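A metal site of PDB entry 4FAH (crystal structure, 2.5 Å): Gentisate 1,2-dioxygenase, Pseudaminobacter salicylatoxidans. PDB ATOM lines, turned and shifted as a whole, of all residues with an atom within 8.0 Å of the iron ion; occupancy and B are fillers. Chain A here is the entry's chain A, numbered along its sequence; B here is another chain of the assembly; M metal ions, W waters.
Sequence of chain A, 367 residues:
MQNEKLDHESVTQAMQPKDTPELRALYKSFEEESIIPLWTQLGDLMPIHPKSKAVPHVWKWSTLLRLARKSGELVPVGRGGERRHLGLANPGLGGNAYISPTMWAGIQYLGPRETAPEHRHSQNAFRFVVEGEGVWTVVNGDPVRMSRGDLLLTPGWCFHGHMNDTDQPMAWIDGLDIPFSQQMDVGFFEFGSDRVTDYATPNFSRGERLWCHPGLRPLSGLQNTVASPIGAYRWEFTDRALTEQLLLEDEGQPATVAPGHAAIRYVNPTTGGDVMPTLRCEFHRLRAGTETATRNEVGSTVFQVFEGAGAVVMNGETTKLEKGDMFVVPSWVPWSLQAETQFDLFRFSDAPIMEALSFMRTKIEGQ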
ATOM      1  N   PRO A 117       9.449  24.557  26.301  1.00  0.00           N
ATOM      2  CA  PRO A 117       8.149  25.150  26.655  1.00  0.00           C
ATOM      3  C   PRO A 117       7.274  25.251  25.397  1.00  0.00           C
ATOM      4  O   PRO A 117       7.768  25.055  24.273  1.00  0.00           O
ATOM      5  CB  PRO A 117       8.526  26.521  27.204  1.00  0.00           C
ATOM      6  CG  PRO A 117       9.836  26.850  26.553  1.00  0.00           C
ATOM      7  CD  PRO A 117      10.540  25.553  26.286  1.00  0.00           C
ATOM      8  N   GLU A 118       5.980  25.521  25.592  1.00  0.00           N
ATOM      9  CA  GLU A 118       5.057  25.709  24.497  1.00  0.00           C
ATOM     10  C   GLU A 118       5.190  27.047  23.790  1.00  0.00           C
ATOM     11  O   GLU A 118       5.409  28.095  24.414  1.00  0.00           O
ATOM     12  CB  GLU A 118       3.638  25.594  24.984  1.00  0.00           C
ATOM     13  CG  GLU A 118       3.264  24.218  25.311  1.00  0.00           C
ATOM     14  CD  GLU A 118       2.023  24.136  26.153  1.00  0.00           C
ATOM     15  OE1 GLU A 118       1.118  25.039  26.032  1.00  0.00           O
ATOM     16  OE2 GLU A 118       1.940  23.145  26.911  1.00  0.00           O
ATOM     17  N   HIS A 119       5.031  26.991  22.473  1.00  0.00           N
ATOM     18  CA  HIS A 119       4.873  28.173  21.628  1.00  0.00           C
ATOM     19  C   HIS A 119       3.909  27.783  20.533  1.00  0.00           C
ATOM     20  O   HIS A 119       3.452  26.617  20.500  1.00  0.00           O
ATOM     21  CB  HIS A 119       6.233  28.641  21.084  1.00  0.00           C
ATOM     22  CG  HIS A 119       6.869  27.707  20.123  1.00  0.00           C
ATOM     23  ND1 HIS A 119       8.240  27.537  20.056  1.00  0.00           N
ATOM     24  CD2 HIS A 119       6.358  26.927  19.154  1.00  0.00           C
ATOM     25  CE1 HIS A 119       8.538  26.660  19.112  1.00  0.00           C
ATOM     26  NE2 HIS A 119       7.411  26.284  18.534  1.00  0.00           N
ATOM     27  N   ARG A 120       3.580  28.726  19.671  1.00  0.00           N
ATOM     28  CA  ARG A 120       2.722  28.499  18.527  1.00  0.00           C
ATOM     29  C   ARG A 120       3.172  29.449  17.421  1.00  0.00           C
ATOM     30  O   ARG A 120       3.672  30.507  17.692  1.00  0.00           O
ATOM     31  CB  ARG A 120       1.259  28.674  18.917  1.00  0.00           C
ATOM     32  CG  ARG A 120       0.656  29.978  18.589  1.00  0.00           C
ATOM     33  CD  ARG A 120      -0.244  30.527  19.635  1.00  0.00           C
ATOM     34  NE  ARG A 120      -1.624  30.153  19.412  1.00  0.00           N
ATOM     35  CZ  ARG A 120      -2.680  30.889  19.718  1.00  0.00           C
ATOM     36  NH1 ARG A 120      -3.883  30.428  19.475  1.00  0.00           N
ATOM     37  NH2 ARG A 120      -2.553  32.083  20.238  1.00  0.00           N
ATOM     38  N   HIS A 121       3.044  29.032  16.183  1.00  0.00           N
ATOM     39  CA  HIS A 121       3.429  29.826  15.025  1.00  0.00           C
ATOM     40  C   HIS A 121       2.496  29.493  13.867  1.00  0.00           C
ATOM     41  O   HIS A 121       1.916  28.413  13.843  1.00  0.00           O
ATOM     42  CB  HIS A 121       4.906  29.617  14.636  1.00  0.00           C
ATOM     43  CG  HIS A 121       5.427  28.227  14.875  1.00  0.00           C
ATOM     44  ND1 HIS A 121       5.193  27.170  13.997  1.00  0.00           N
ATOM     45  CD2 HIS A 121       6.232  27.727  15.843  1.00  0.00           C
ATOM     46  CE1 HIS A 121       5.801  26.086  14.443  1.00  0.00           C
ATOM     47  NE2 HIS A 121       6.443  26.391  15.564  1.00  0.00           N
ATOM     48  N   GLN A 123       3.397  28.909  10.771  1.00  0.00           N
ATOM     49  CA  GLN A 123       4.120  27.921   9.903  1.00  0.00           C
ATOM     50  C   GLN A 123       3.734  26.519  10.291  1.00  0.00           C
ATOM     51  O   GLN A 123       3.786  26.237  11.476  1.00  0.00           O
ATOM     52  CB  GLN A 123       5.643  28.004  10.094  1.00  0.00           C
ATOM     53  CG  GLN A 123       6.305  29.290   9.575  1.00  0.00           C
ATOM     54  CD  GLN A 123       6.288  30.452  10.573  1.00  0.00           C
ATOM     55  OE1 GLN A 123       7.112  31.364  10.502  1.00  0.00           O
ATOM     56  NE2 GLN A 123       5.348  30.425  11.498  1.00  0.00           N
ATOM     57  N   ALA A 125       4.051  22.285  10.601  1.00  0.00           N
ATOM     58  CA  ALA A 125       5.190  21.413  10.936  1.00  0.00           C
ATOM     59  C   ALA A 125       4.796  19.954  11.285  1.00  0.00           C
ATOM     60  O   ALA A 125       3.682  19.704  11.758  1.00  0.00           O
ATOM     61  CB  ALA A 125       5.996  22.025  12.079  1.00  0.00           C
ATOM     62  N   ARG A 127       6.744  16.011  12.860  1.00  0.00           N
ATOM     63  CA  ARG A 127       7.886  15.358  13.506  1.00  0.00           C
ATOM     64  C   ARG A 127       7.829  13.890  13.092  1.00  0.00           C
ATOM     65  O   ARG A 127       6.851  13.214  13.373  1.00  0.00           O
ATOM     66  CB  ARG A 127       7.796  15.487  15.024  1.00  0.00           C
ATOM     67  CG  ARG A 127       7.789  16.953  15.471  1.00  0.00           C
ATOM     68  CD  ARG A 127       7.529  17.206  16.950  1.00  0.00           C
ATOM     69  NE  ARG A 127       7.707  18.620  17.224  1.00  0.00           N
ATOM     70  CZ  ARG A 127       7.916  19.157  18.422  1.00  0.00           C
ATOM     71  NH1 ARG A 127       7.964  18.389  19.498  1.00  0.00           N
ATOM     72  NH2 ARG A 127       8.139  20.468  18.531  1.00  0.00           N
ATOM     73  N   THR A 154       2.218  19.030  14.099  1.00  0.00           N
ATOM     74  CA  THR A 154       1.934  20.161  15.008  1.00  0.00           C
ATOM     75  C   THR A 154       1.484  21.239  14.076  1.00  0.00           C
ATOM     76  O   THR A 154       2.282  22.039  13.620  1.00  0.00           O
ATOM     77  CB  THR A 154       3.177  20.587  15.889  1.00  0.00           C
ATOM     78  OG1 THR A 154       4.225  21.107  15.058  1.00  0.00           O
ATOM     79  CG2 THR A 154       3.717  19.427  16.679  1.00  0.00           C
ATOM     80  N   CYS A 158      -1.191  25.717  16.463  1.00  0.00           N
ATOM     81  CA  CYS A 158      -1.347  24.814  17.594  1.00  0.00           C
ATOM     82  C   CYS A 158      -0.172  24.960  18.560  1.00  0.00           C
ATOM     83  O   CYS A 158       0.995  24.794  18.168  1.00  0.00           O
ATOM     84  CB  CYS A 158      -1.439  23.352  17.118  1.00  0.00           C
ATOM     85  SG  CYS A 158      -3.015  23.051  16.165  1.00  0.00           S
ATOM     86  N   PHE A 159      -0.485  25.266  19.821  1.00  0.00           N
ATOM     87  CA  PHE A 159       0.515  25.311  20.888  1.00  0.00           C
ATOM     88  C   PHE A 159       1.174  23.958  20.959  1.00  0.00           C
ATOM     89  O   PHE A 159       0.502  22.916  20.947  1.00  0.00           O
ATOM     90  CB  PHE A 159      -0.094  25.673  22.264  1.00  0.00           C
ATOM     91  CG  PHE A 159      -0.423  27.140  22.429  1.00  0.00           C
ATOM     92  CD1 PHE A 159       0.591  28.083  22.596  1.00  0.00           C
ATOM     93  CD2 PHE A 159      -1.725  27.563  22.429  1.00  0.00           C
ATOM     94  CE1 PHE A 159       0.300  29.484  22.776  1.00  0.00           C
ATOM     95  CE2 PHE A 159      -2.035  28.929  22.589  1.00  0.00           C
ATOM     96  CZ  PHE A 159      -0.988  29.898  22.773  1.00  0.00           C
ATOM     97  N   HIS A 160       2.500  23.945  20.987  1.00  0.00           N
ATOM     98  CA  HIS A 160       3.206  22.686  21.108  1.00  0.00           C
ATOM     99  C   HIS A 160       4.472  22.878  21.925  1.00  0.00           C
ATOM    100  O   HIS A 160       5.126  23.938  21.848  1.00  0.00           O
ATOM    101  CB  HIS A 160       3.538  22.104  19.711  1.00  0.00           C
ATOM    102  CG  HIS A 160       4.281  23.047  18.823  1.00  0.00           C
ATOM    103  ND1 HIS A 160       3.640  23.957  18.017  1.00  0.00           N
ATOM    104  CD2 HIS A 160       5.606  23.250  18.630  1.00  0.00           C
ATOM    105  CE1 HIS A 160       4.532  24.667  17.352  1.00  0.00           C
ATOM    106  NE2 HIS A 160       5.736  24.262  17.715  1.00  0.00           N
ATOM    107  N   GLY A 161       4.795  21.847  22.708  1.00  0.00           N
ATOM    108  CA  GLY A 161       6.035  21.687  23.435  1.00  0.00           C
ATOM    109  C   GLY A 161       6.285  20.218  23.735  1.00  0.00           C
ATOM    110  O   GLY A 161       5.504  19.345  23.393  1.00  0.00           O
ATOM    111  N   HIS A 162       7.384  19.905  24.387  1.00  0.00           N
ATOM    112  CA  HIS A 162       7.656  18.489  24.623  1.00  0.00           C
ATOM    113  C   HIS A 162       8.445  18.202  25.889  1.00  0.00           C
ATOM    114  O   HIS A 162       9.096  19.098  26.423  1.00  0.00           O
ATOM    115  CB  HIS A 162       8.378  17.875  23.410  1.00  0.00           C
ATOM    116  CG  HIS A 162       9.640  18.572  23.036  1.00  0.00           C
ATOM    117  ND1 HIS A 162       9.717  19.429  21.974  1.00  0.00           N
ATOM    118  CD2 HIS A 162      10.882  18.515  23.566  1.00  0.00           C
ATOM    119  CE1 HIS A 162      10.954  19.896  21.870  1.00  0.00           C
ATOM    120  NE2 HIS A 162      11.672  19.369  22.832  1.00  0.00           N
ATOM    121  N   ASP A 174      12.460  17.191  11.741  1.00  0.00           N
ATOM    122  CA  ASP A 174      11.543  18.325  11.870  1.00  0.00           C
ATOM    123  C   ASP A 174      11.348  18.879  10.513  1.00  0.00           C
ATOM    124  O   ASP A 174      12.298  19.473   9.960  1.00  0.00           O
ATOM    125  CB  ASP A 174      12.194  19.503  12.627  1.00  0.00           C
ATOM    126  CG  ASP A 174      11.773  19.620  14.063  1.00  0.00           C
ATOM    127  OD1 ASP A 174      10.585  19.423  14.435  1.00  0.00           O
ATOM    128  OD2 ASP A 174      12.687  19.932  14.830  1.00  0.00           O
ATOM    129  N   LEU A 176       9.295  21.631   8.288  1.00  0.00           N
ATOM    130  CA  LEU A 176       8.402  22.763   8.330  1.00  0.00           C
ATOM    131  C   LEU A 176       8.290  23.480   6.989  1.00  0.00           C
ATOM    132  O   LEU A 176       9.112  23.243   6.088  1.00  0.00           O
ATOM    133  CB  LEU A 176       8.832  23.787   9.390  1.00  0.00           C
ATOM    134  CG  LEU A 176       9.049  23.385  10.852  1.00  0.00           C
ATOM    135  CD1 LEU A 176      10.533  23.119  11.106  1.00  0.00           C
ATOM    136  CD2 LEU A 176       8.565  24.531  11.661  1.00  0.00           C
ATOM    137  N   ILE A 178       8.768  26.713   6.796  1.00  0.00           N
ATOM    138  CA  ILE A 178       9.567  27.937   7.019  1.00  0.00           C
ATOM    139  C   ILE A 178      10.012  28.694   5.744  1.00  0.00           C
ATOM    140  O   ILE A 178       9.609  29.825   5.602  1.00  0.00           O
ATOM    141  CB  ILE A 178      10.738  27.701   8.054  1.00  0.00           C
ATOM    142  CG1 ILE A 178      10.185  27.774   9.470  1.00  0.00           C
ATOM    143  CG2 ILE A 178      11.861  28.754   7.903  1.00  0.00           C
ATOM    144  CD1 ILE A 178      11.091  27.211  10.492  1.00  0.00           C
ATOM    145  N   PHE A 189       3.966  34.335  15.465  1.00  0.00           N
ATOM    146  CA  PHE A 189       4.577  33.542  16.552  1.00  0.00           C
ATOM    147  C   PHE A 189       4.095  34.017  17.941  1.00  0.00           C
ATOM    148  O   PHE A 189       3.935  35.230  18.165  1.00  0.00           O
ATOM    149  CB  PHE A 189       6.105  33.620  16.469  1.00  0.00           C
ATOM    150  CG  PHE A 189       6.803  32.879  17.560  1.00  0.00           C
ATOM    151  CD1 PHE A 189       6.937  33.438  18.844  1.00  0.00           C
ATOM    152  CD2 PHE A 189       7.341  31.616  17.324  1.00  0.00           C
ATOM    153  CE1 PHE A 189       7.595  32.715  19.876  1.00  0.00           C
ATOM    154  CE2 PHE A 189       7.964  30.899  18.330  1.00  0.00           C
ATOM    155  CZ  PHE A 189       8.113  31.449  19.612  1.00  0.00           C
ATOM    156  N   MET B  46      11.313  32.950  13.019  1.00  0.00           N
ATOM    157  CA  MET B  46       9.857  32.907  13.075  1.00  0.00           C
ATOM    158  C   MET B  46       9.416  34.213  13.723  1.00  0.00           C
ATOM    159  O   MET B  46       9.278  34.306  14.935  1.00  0.00           O
ATOM    160  CB  MET B  46       9.366  31.671  13.852  1.00  0.00           C
ATOM    161  CG  MET B  46       9.813  30.377  13.199  1.00  0.00           C
ATOM    162  SD  MET B  46       9.099  28.899  13.896  1.00  0.00           S
ATOM    163  CE  MET B  46       9.871  28.983  15.531  1.00  0.00           C
HETATM  164 FE    FE M   1       7.578  25.035  16.929  1.00  0.00          FE
HETATM  165  O   HOH W   1       9.699  25.680  16.275  1.00  0.00           O
HETATM  166  O   HOH W   2       9.185  23.625  17.692  1.00  0.00           O
HETATM  167  O   HOH W   3       8.372  23.554  15.299  1.00  0.00           O
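A ring nitrogen (ND1) of His 160 lies within hydrogen-bond range of the backbone carbonyl oxygen (O) of Cys 158. ND1 of His 121 is in hydrogen-bond range of O of Gln 123, at 3.0 Å.
Three residues have an atom within 4 Å of the iron ion: His 119, His 121 and His 160.
The iron ion is bound by NE2 of His 119, 2.0 Å away. The iron ion is bound by NE2 of His 160 (2.1 Å). The iron ion is bound by NE2 of His 121 (2.2 Å). Water W2 is bound to the iron ion (2.3 Å). The iron ion is bound by water W1, 2.3 Å away. Water W3 binds the iron ion (2.3 Å). The iron ion has six donor atoms within binding distance.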
